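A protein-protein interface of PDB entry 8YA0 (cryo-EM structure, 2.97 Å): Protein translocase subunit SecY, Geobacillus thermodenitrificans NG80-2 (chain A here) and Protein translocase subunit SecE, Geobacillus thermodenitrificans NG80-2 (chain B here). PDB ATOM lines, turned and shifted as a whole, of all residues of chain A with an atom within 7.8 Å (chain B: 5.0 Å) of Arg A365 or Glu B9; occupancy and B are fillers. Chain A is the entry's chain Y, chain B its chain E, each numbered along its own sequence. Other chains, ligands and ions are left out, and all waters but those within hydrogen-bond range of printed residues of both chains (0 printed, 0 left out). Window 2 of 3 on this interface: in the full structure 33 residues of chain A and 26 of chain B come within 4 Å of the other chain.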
ATOM      1  N   ARG A 238       5.332  18.017  14.101  1.00  0.00           N
ATOM      2  CA  ARG A 238       4.537  16.890  13.655  1.00  0.00           C
ATOM      3  C   ARG A 238       4.180  16.092  14.892  1.00  0.00           C
ATOM      4  O   ARG A 238       5.059  15.578  15.574  1.00  0.00           O
ATOM      5  CB  ARG A 238       5.314  16.054  12.656  1.00  0.00           C
ATOM      6  CG  ARG A 238       4.806  14.685  12.479  1.00  0.00           C
ATOM      7  CD  ARG A 238       3.629  14.663  11.604  1.00  0.00           C
ATOM      8  NE  ARG A 238       3.413  13.328  11.096  1.00  0.00           N
ATOM      9  CZ  ARG A 238       2.577  12.467  11.639  1.00  0.00           C
ATOM     10  NH1 ARG A 238       1.873  12.816  12.691  1.00  0.00           N
ATOM     11  NH2 ARG A 238       2.435  11.266  11.124  1.00  0.00           N
ATOM     12  N   VAL A 265      10.219  20.126  13.038  1.00  0.00           N
ATOM     13  CA  VAL A 265      10.606  20.017  11.642  1.00  0.00           C
ATOM     14  C   VAL A 265      12.110  20.161  11.508  1.00  0.00           C
ATOM     15  O   VAL A 265      12.728  19.496  10.680  1.00  0.00           O
ATOM     16  CB  VAL A 265       9.852  21.047  10.801  1.00  0.00           C
ATOM     17  CG1 VAL A 265       9.999  20.744   9.374  1.00  0.00           C
ATOM     18  CG2 VAL A 265       8.428  20.986  11.137  1.00  0.00           C
ATOM     19  N   TYR A 323      20.962  15.422   8.642  1.00  0.00           N
ATOM     20  CA  TYR A 323      20.419  14.071   8.727  1.00  0.00           C
ATOM     21  C   TYR A 323      21.087  13.269   9.828  1.00  0.00           C
ATOM     22  O   TYR A 323      20.401  12.619  10.630  1.00  0.00           O
ATOM     23  CB  TYR A 323      20.562  13.368   7.397  1.00  0.00           C
ATOM     24  CG  TYR A 323      19.337  13.508   6.578  1.00  0.00           C
ATOM     25  CD1 TYR A 323      18.327  12.601   6.681  1.00  0.00           C
ATOM     26  CD2 TYR A 323      19.180  14.565   5.720  1.00  0.00           C
ATOM     27  CE1 TYR A 323      17.210  12.728   5.951  1.00  0.00           C
ATOM     28  CE2 TYR A 323      18.061  14.695   4.979  1.00  0.00           C
ATOM     29  CZ  TYR A 323      17.081  13.771   5.104  1.00  0.00           C
ATOM     30  OH  TYR A 323      15.940  13.877   4.374  1.00  0.00           O
ATOM     31  N   PHE A 327      19.112  12.206  13.459  1.00  0.00           N
ATOM     32  CA  PHE A 327      18.985  10.854  13.974  1.00  0.00           C
ATOM     33  C   PHE A 327      19.791  10.622  15.235  1.00  0.00           C
ATOM     34  O   PHE A 327      19.572   9.625  15.915  1.00  0.00           O
ATOM     35  CB  PHE A 327      19.392   9.858  12.914  1.00  0.00           C
ATOM     36  CG  PHE A 327      18.321   9.578  11.947  1.00  0.00           C
ATOM     37  CD1 PHE A 327      18.034  10.467  10.944  1.00  0.00           C
ATOM     38  CD2 PHE A 327      17.574   8.439  12.053  1.00  0.00           C
ATOM     39  CE1 PHE A 327      17.036  10.217  10.064  1.00  0.00           C
ATOM     40  CE2 PHE A 327      16.578   8.190  11.172  1.00  0.00           C
ATOM     41  CZ  PHE A 327      16.307   9.082  10.186  1.00  0.00           C
ATOM     42  N   GLU A 357      10.623   1.934  12.851  1.00  0.00           N
ATOM     43  CA  GLU A 357      10.673   2.297  11.451  1.00  0.00           C
ATOM     44  C   GLU A 357       9.555   3.239  11.034  1.00  0.00           C
ATOM     45  O   GLU A 357       9.750   3.999  10.087  1.00  0.00           O
ATOM     46  CB  GLU A 357      10.692   1.052  10.596  1.00  0.00           C
ATOM     47  CG  GLU A 357       9.438   0.305  10.577  1.00  0.00           C
ATOM     48  CD  GLU A 357       9.611  -1.041   9.948  1.00  0.00           C
ATOM     49  OE1 GLU A 357      10.726  -1.589  10.039  1.00  0.00           O
ATOM     50  OE2 GLU A 357       8.632  -1.553   9.367  1.00  0.00           O
ATOM     51  N   TYR A 358       8.440   3.289  11.760  1.00  0.00           N
ATOM     52  CA  TYR A 358       7.438   4.324  11.519  1.00  0.00           C
ATOM     53  C   TYR A 358       7.995   5.713  11.786  1.00  0.00           C
ATOM     54  O   TYR A 358       7.912   6.611  10.935  1.00  0.00           O
ATOM     55  CB  TYR A 358       6.229   4.060  12.403  1.00  0.00           C
ATOM     56  CG  TYR A 358       5.064   4.977  12.211  1.00  0.00           C
ATOM     57  CD1 TYR A 358       4.094   4.689  11.296  1.00  0.00           C
ATOM     58  CD2 TYR A 358       4.911   6.102  12.981  1.00  0.00           C
ATOM     59  CE1 TYR A 358       3.029   5.508  11.132  1.00  0.00           C
ATOM     60  CE2 TYR A 358       3.857   6.926  12.815  1.00  0.00           C
ATOM     61  CZ  TYR A 358       2.919   6.622  11.893  1.00  0.00           C
ATOM     62  OH  TYR A 358       1.848   7.444  11.724  1.00  0.00           O
ATOM     63  N   VAL A 359       8.581   5.915  12.959  1.00  0.00           N
ATOM     64  CA  VAL A 359       9.081   7.240  13.257  1.00  0.00           C
ATOM     65  C   VAL A 359      10.397   7.515  12.541  1.00  0.00           C
ATOM     66  O   VAL A 359      10.741   8.679  12.327  1.00  0.00           O
ATOM     67  CB  VAL A 359       9.123   7.405  14.780  1.00  0.00           C
ATOM     68  CG1 VAL A 359      10.213   6.670  15.337  1.00  0.00           C
ATOM     69  CG2 VAL A 359       9.264   8.824  15.145  1.00  0.00           C
ATOM     70  N   THR A 360      11.088   6.493  12.046  1.00  0.00           N
ATOM     71  CA  THR A 360      12.203   6.720  11.134  1.00  0.00           C
ATOM     72  C   THR A 360      11.738   7.303   9.808  1.00  0.00           C
ATOM     73  O   THR A 360      12.366   8.225   9.286  1.00  0.00           O
ATOM     74  CB  THR A 360      12.955   5.415  10.934  1.00  0.00           C
ATOM     75  OG1 THR A 360      13.624   5.081  12.143  1.00  0.00           O
ATOM     76  CG2 THR A 360      13.956   5.513   9.885  1.00  0.00           C
ATOM     77  N   ARG A 361      10.623   6.827   9.272  1.00  0.00           N
ATOM     78  CA  ARG A 361      10.123   7.411   8.032  1.00  0.00           C
ATOM     79  C   ARG A 361       9.641   8.846   8.223  1.00  0.00           C
ATOM     80  O   ARG A 361       9.906   9.716   7.370  1.00  0.00           O
ATOM     81  CB  ARG A 361       9.017   6.543   7.480  1.00  0.00           C
ATOM     82  CG  ARG A 361       9.499   5.199   7.079  1.00  0.00           C
ATOM     83  CD  ARG A 361       8.500   4.506   6.220  1.00  0.00           C
ATOM     84  NE  ARG A 361       7.285   4.178   6.945  1.00  0.00           N
ATOM     85  CZ  ARG A 361       7.030   2.983   7.456  1.00  0.00           C
ATOM     86  NH1 ARG A 361       7.913   2.009   7.321  1.00  0.00           N
ATOM     87  NH2 ARG A 361       5.900   2.762   8.104  1.00  0.00           N
ATOM     88  N   ILE A 362       8.952   9.110   9.337  1.00  0.00           N
ATOM     89  CA  ILE A 362       8.557  10.480   9.677  1.00  0.00           C
ATOM     90  C   ILE A 362       9.773  11.386   9.755  1.00  0.00           C
ATOM     91  O   ILE A 362       9.776  12.498   9.216  1.00  0.00           O
ATOM     92  CB  ILE A 362       7.788  10.504  11.008  1.00  0.00           C
ATOM     93  CG1 ILE A 362       6.573   9.593  10.977  1.00  0.00           C
ATOM     94  CG2 ILE A 362       7.403  11.891  11.369  1.00  0.00           C
ATOM     95  CD1 ILE A 362       5.498  10.037  10.096  1.00  0.00           C
ATOM     96  N   LEU A 363      10.843  10.894  10.365  1.00  0.00           N
ATOM     97  CA  LEU A 363      12.030  11.700  10.567  1.00  0.00           C
ATOM     98  C   LEU A 363      12.789  11.948   9.283  1.00  0.00           C
ATOM     99  O   LEU A 363      13.397  13.005   9.143  1.00  0.00           O
ATOM    100  CB  LEU A 363      12.927  11.020  11.574  1.00  0.00           C
ATOM    101  CG  LEU A 363      13.844  11.921  12.354  1.00  0.00           C
ATOM    102  CD1 LEU A 363      13.048  12.978  13.015  1.00  0.00           C
ATOM    103  CD2 LEU A 363      14.496  11.067  13.350  1.00  0.00           C
ATOM    104  N   TYR A 364      12.758  11.015   8.336  1.00  0.00           N
ATOM    105  CA  TYR A 364      13.378  11.256   7.034  1.00  0.00           C
ATOM    106  C   TYR A 364      12.710  12.410   6.303  1.00  0.00           C
ATOM    107  O   TYR A 364      13.385  13.309   5.784  1.00  0.00           O
ATOM    108  CB  TYR A 364      13.311  10.005   6.179  1.00  0.00           C
ATOM    109  CG  TYR A 364      14.415   9.047   6.442  1.00  0.00           C
ATOM    110  CD1 TYR A 364      15.700   9.483   6.607  1.00  0.00           C
ATOM    111  CD2 TYR A 364      14.169   7.700   6.525  1.00  0.00           C
ATOM    112  CE1 TYR A 364      16.720   8.601   6.838  1.00  0.00           C
ATOM    113  CE2 TYR A 364      15.176   6.812   6.767  1.00  0.00           C
ATOM    114  CZ  TYR A 364      16.448   7.267   6.932  1.00  0.00           C
ATOM    115  OH  TYR A 364      17.459   6.374   7.174  1.00  0.00           O
ATOM    116  N   ARG A 365      11.380  12.437   6.298  1.00  0.00           N
ATOM    117  CA  ARG A 365      10.708  13.506   5.561  1.00  0.00           C
ATOM    118  C   ARG A 365      10.844  14.870   6.247  1.00  0.00           C
ATOM    119  O   ARG A 365      11.167  15.892   5.598  1.00  0.00           O
ATOM    120  CB  ARG A 365       9.261  13.126   5.367  1.00  0.00           C
ATOM    121  CG  ARG A 365       9.150  11.787   4.725  1.00  0.00           C
ATOM    122  CD  ARG A 365       7.821  11.213   4.982  1.00  0.00           C
ATOM    123  NE  ARG A 365       7.735   9.838   4.544  1.00  0.00           N
ATOM    124  CZ  ARG A 365       6.801   9.008   4.972  1.00  0.00           C
ATOM    125  NH1 ARG A 365       5.907   9.433   5.844  1.00  0.00           N
ATOM    126  NH2 ARG A 365       6.762   7.759   4.540  1.00  0.00           N
ATOM    127  N   LEU A 366      10.638  14.908   7.563  1.00  0.00           N
ATOM    128  CA  LEU A 366      10.794  16.161   8.287  1.00  0.00           C
ATOM    129  C   LEU A 366      12.221  16.669   8.256  1.00  0.00           C
ATOM    130  O   LEU A 366      12.441  17.879   8.213  1.00  0.00           O
ATOM    131  CB  LEU A 366      10.372  15.995   9.731  1.00  0.00           C
ATOM    132  CG  LEU A 366       8.938  15.672  10.048  1.00  0.00           C
ATOM    133  CD1 LEU A 366       8.822  15.845  11.501  1.00  0.00           C
ATOM    134  CD2 LEU A 366       8.010  16.588   9.324  1.00  0.00           C
ATOM    135  N   THR A 367      13.200  15.773   8.256  1.00  0.00           N
ATOM    136  CA  THR A 367      14.580  16.206   8.246  1.00  0.00           C
ATOM    137  C   THR A 367      14.972  16.738   6.882  1.00  0.00           C
ATOM    138  O   THR A 367      15.824  17.620   6.805  1.00  0.00           O
ATOM    139  CB  THR A 367      15.457  15.042   8.683  1.00  0.00           C
ATOM    140  OG1 THR A 367      15.052  14.643   9.986  1.00  0.00           O
ATOM    141  CG2 THR A 367      16.879  15.431   8.797  1.00  0.00           C
ATOM    142  N   LEU A 368      14.336  16.265   5.804  1.00  0.00           N
ATOM    143  CA  LEU A 368      14.571  16.891   4.502  1.00  0.00           C
ATOM    144  C   LEU A 368      14.162  18.350   4.507  1.00  0.00           C
ATOM    145  O   LEU A 368      14.943  19.225   4.107  1.00  0.00           O
ATOM    146  CB  LEU A 368      13.822  16.163   3.400  1.00  0.00           C
ATOM    147  CG  LEU A 368      13.898  16.890   2.065  1.00  0.00           C
ATOM    148  CD1 LEU A 368      15.284  16.806   1.510  1.00  0.00           C
ATOM    149  CD2 LEU A 368      12.929  16.315   1.098  1.00  0.00           C
ATOM    150  N   VAL A 369      12.959  18.636   5.005  1.00  0.00           N
ATOM    151  CA  VAL A 369      12.514  20.035   5.026  1.00  0.00           C
ATOM    152  C   VAL A 369      13.363  20.884   5.973  1.00  0.00           C
ATOM    153  O   VAL A 369      13.791  21.990   5.617  1.00  0.00           O
ATOM    154  CB  VAL A 369      11.024  20.108   5.372  1.00  0.00           C
ATOM    155  CG1 VAL A 369      10.630  21.494   5.770  1.00  0.00           C
ATOM    156  CG2 VAL A 369      10.245  19.684   4.181  1.00  0.00           C
ATOM    157  N   GLY A 370      13.684  20.362   7.154  1.00  0.00           N
ATOM    158  CA  GLY A 370      14.495  21.116   8.095  1.00  0.00           C
ATOM    159  C   GLY A 370      15.925  21.326   7.655  1.00  0.00           C
ATOM    160  O   GLY A 370      16.506  22.371   7.929  1.00  0.00           O
ATOM    161  N   SER A 371      16.493  20.374   6.920  1.00  0.00           N
ATOM    162  CA  SER A 371      17.854  20.517   6.423  1.00  0.00           C
ATOM    163  C   SER A 371      17.931  21.523   5.297  1.00  0.00           C
ATOM    164  O   SER A 371      18.900  22.277   5.213  1.00  0.00           O
ATOM    165  CB  SER A 371      18.373  19.181   5.937  1.00  0.00           C
ATOM    166  OG  SER A 371      17.589  18.719   4.870  1.00  0.00           O
ATOM    167  N   ASN B   5       8.078   9.541  -5.904  1.00  0.00           N
ATOM    168  CA  ASN B   5       7.224   8.996  -4.857  1.00  0.00           C
ATOM    169  C   ASN B   5       7.653   9.488  -3.480  1.00  0.00           C
ATOM    170  O   ASN B   5       6.805   9.817  -2.644  1.00  0.00           O
ATOM    171  CB  ASN B   5       7.246   7.474  -4.914  1.00  0.00           C
ATOM    172  CG  ASN B   5       5.957   6.861  -4.429  1.00  0.00           C
ATOM    173  OD1 ASN B   5       5.507   7.135  -3.318  1.00  0.00           O
ATOM    174  ND2 ASN B   5       5.349   6.029  -5.266  1.00  0.00           N
ATOM    175  N   PHE B   6       8.966   9.587  -3.244  1.00  0.00           N
ATOM    176  CA  PHE B   6       9.448  10.109  -1.969  1.00  0.00           C
ATOM    177  C   PHE B   6       9.087  11.572  -1.793  1.00  0.00           C
ATOM    178  O   PHE B   6       8.734  11.992  -0.688  1.00  0.00           O
ATOM    179  CB  PHE B   6      10.956   9.947  -1.843  1.00  0.00           C
ATOM    180  CG  PHE B   6      11.541  10.685  -0.670  1.00  0.00           C
ATOM    181  CD1 PHE B   6      11.228  10.314   0.618  1.00  0.00           C
ATOM    182  CD2 PHE B   6      12.392  11.750  -0.853  1.00  0.00           C
ATOM    183  CE1 PHE B   6      11.757  10.989   1.694  1.00  0.00           C
ATOM    184  CE2 PHE B   6      12.919  12.423   0.232  1.00  0.00           C
ATOM    185  CZ  PHE B   6      12.601  12.037   1.498  1.00  0.00           C
ATOM    186  N   PHE B   7       9.155  12.365  -2.858  1.00  0.00           N
ATOM    187  CA  PHE B   7       8.807  13.770  -2.709  1.00  0.00           C
ATOM    188  C   PHE B   7       7.306  13.968  -2.566  1.00  0.00           C
ATOM    189  O   PHE B   7       6.868  14.907  -1.887  1.00  0.00           O
ATOM    190  CB  PHE B   7       9.366  14.575  -3.867  1.00  0.00           C
ATOM    191  CG  PHE B   7      10.754  15.051  -3.623  1.00  0.00           C
ATOM    192  CD1 PHE B   7      10.987  16.135  -2.808  1.00  0.00           C
ATOM    193  CD2 PHE B   7      11.829  14.399  -4.182  1.00  0.00           C
ATOM    194  CE1 PHE B   7      12.263  16.566  -2.569  1.00  0.00           C
ATOM    195  CE2 PHE B   7      13.108  14.827  -3.948  1.00  0.00           C
ATOM    196  CZ  PHE B   7      13.326  15.911  -3.140  1.00  0.00           C
ATOM    197  N   LYS B   8       6.506  13.073  -3.142  1.00  0.00           N
ATOM    198  CA  LYS B   8       5.079  13.093  -2.850  1.00  0.00           C
ATOM    199  C   LYS B   8       4.820  12.745  -1.395  1.00  0.00           C
ATOM    200  O   LYS B   8       3.921  13.312  -0.768  1.00  0.00           O
ATOM    201  CB  LYS B   8       4.332  12.135  -3.777  1.00  0.00           C
ATOM    202  CG  LYS B   8       4.210  12.615  -5.224  1.00  0.00           C
ATOM    203  CD  LYS B   8       3.674  14.041  -5.301  1.00  0.00           C
ATOM    204  CE  LYS B   8       4.402  14.864  -6.361  1.00  0.00           C
ATOM    205  NZ  LYS B   8       4.194  16.335  -6.184  1.00  0.00           N
ATOM    206  N   GLU B   9       5.626  11.844  -0.827  1.00  0.00           N
ATOM    207  CA  GLU B   9       5.499  11.532   0.594  1.00  0.00           C
ATOM    208  C   GLU B   9       5.930  12.691   1.478  1.00  0.00           C
ATOM    209  O   GLU B   9       5.354  12.884   2.544  1.00  0.00           O
ATOM    210  CB  GLU B   9       6.316  10.297   0.945  1.00  0.00           C
ATOM    211  CG  GLU B   9       5.803   9.015   0.351  1.00  0.00           C
ATOM    212  CD  GLU B   9       4.858   8.265   1.263  1.00  0.00           C
ATOM    213  OE1 GLU B   9       4.081   8.912   1.994  1.00  0.00           O
ATOM    214  OE2 GLU B   9       4.890   7.017   1.247  1.00  0.00           O
ATOM    215  N   VAL B  10       6.935  13.459   1.061  1.00  0.00           N
ATOM    216  CA  VAL B  10       7.358  14.623   1.836  1.00  0.00           C
ATOM    217  C   VAL B  10       6.269  15.680   1.842  1.00  0.00           C
ATOM    218  O   VAL B  10       5.965  16.271   2.888  1.00  0.00           O
ATOM    219  CB  VAL B  10       8.674  15.188   1.286  1.00  0.00           C
ATOM    220  CG1 VAL B  10       9.046  16.446   1.999  1.00  0.00           C
ATOM    221  CG2 VAL B  10       9.756  14.215   1.470  1.00  0.00           C
ATOM    222  N   VAL B  11       5.647  15.920   0.686  1.00  0.00           N
ATOM    223  CA  VAL B  11       4.562  16.897   0.619  1.00  0.00           C
ATOM    224  C   VAL B  11       3.344  16.401   1.389  1.00  0.00           C
ATOM    225  O   VAL B  11       2.656  17.181   2.053  1.00  0.00           O
ATOM    226  CB  VAL B  11       4.241  17.215  -0.850  1.00  0.00           C
ATOM    227  CG1 VAL B  11       3.038  18.107  -0.976  1.00  0.00           C
ATOM    228  CG2 VAL B  11       5.426  17.881  -1.485  1.00  0.00           C
ATOM    229  N   ARG B  12       3.100  15.093   1.375  1.00  0.00           N
ATOM    230  CA  ARG B  12       2.024  14.531   2.181  1.00  0.00           C
ATOM    231  C   ARG B  12       2.314  14.634   3.668  1.00  0.00           C
ATOM    232  O   ARG B  12       1.390  14.805   4.466  1.00  0.00           O
ATOM    233  CB  ARG B  12       1.813  13.077   1.793  1.00  0.00           C
ATOM    234  CG  ARG B  12       0.438  12.542   2.049  1.00  0.00           C
ATOM    235  CD  ARG B  12       0.251  11.286   1.237  1.00  0.00           C
ATOM    236  NE  ARG B  12       0.675  11.496  -0.145  1.00  0.00           N
ATOM    237  CZ  ARG B  12       1.106  10.535  -0.953  1.00  0.00           C
ATOM    238  NH1 ARG B  12       1.185   9.284  -0.523  1.00  0.00           N
ATOM    239  NH2 ARG B  12       1.468  10.825  -2.193  1.00  0.00           N
ATOM    240  N   GLU B  13       3.584  14.535   4.050  1.00  0.00           N
ATOM    241  CA  GLU B  13       3.981  14.649   5.443  1.00  0.00           C
ATOM    242  C   GLU B  13       3.863  16.068   5.945  1.00  0.00           C
ATOM    243  O   GLU B  13       3.524  16.280   7.108  1.00  0.00           O
ATOM    244  CB  GLU B  13       5.411  14.170   5.609  1.00  0.00           C
ATOM    245  CG  GLU B  13       5.851  14.033   7.024  1.00  0.00           C
ATOM    246  CD  GLU B  13       5.162  12.902   7.709  1.00  0.00           C
ATOM    247  OE1 GLU B  13       4.476  13.143   8.718  1.00  0.00           O
ATOM    248  OE2 GLU B  13       5.300  11.765   7.232  1.00  0.00           O
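OE2 of Glu B13 touches CD1 of Ile A362, at 3.4 Å.
Phe B6 touches Leu A368.
Leu A368 touches Phe B7.
Leu A368 touches Val B10 (CD2 to CG2, 3.8 Å).
The guanidinium group (NE) of Arg A238 lies within salt-bridge range of the side-chain carboxylate (OE1) of Glu B13 (2.6 Å).
The guanidinium group (NH2) of Arg A365 lies within salt-bridge range of the side-chain carboxylate (OE2) of Glu B9 (3.9 Å).
The guanidinium group of Arg A365 lies within salt-bridge range of the side-chain carboxylate of Glu B13 (2.8 Å).
Of the 19 printed residues of chain A, 4 touch a printed residue of chain B.
Hydrophobic or aromatic side chains of chain A within 4 Å of the printed part of chain B: Ile A362 and Leu A368.
Along chain A the printed residues that touch a printed residue of chain B span positions 238 to 368.
Among the printed residues, Asp or Glu carboxylates within 4 Å of a Lys or Arg side-chain nitrogen of the other chain: Arg A238 with Glu B13, Arg A365 with Glu B9 and Arg A365 with Glu B13.
Arg A365 touches just these residues of chain B: Glu B9 and Glu B13.
Glu B9 touches just one residue of chain A: Arg A365.
Printed residues of chain A within 4 Å of Glu B13: Arg A238, Ile A362 and Arg A365.
Of the printed residues of chain A, Val B10 touches Leu A368 (3.8 Å).
Printed residues of chain A within 4 Å of Phe B7: Leu A368 (3.7 Å).
Lys B8 touches none of the printed residues of chain A.
Tyr A364 touches none of the printed residues of chain B.
The nearest printed residue of chain B that does not touch Ile A362 is Phe B6 (7.9 Å).
OH of Tyr A323 lies within hydrogen-bond range of N of Leu A368 (3.2 Å).
The backbone carbonyl oxygen of Leu A368 sits at hydrogen-bond distance from the side-chain hydroxyl of Ser A371 (2.8 Å).
The side-chain carboxylate (OE1) of Glu B9 is in salt-bridge range of the guanidinium group (NH1) of Arg B12.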
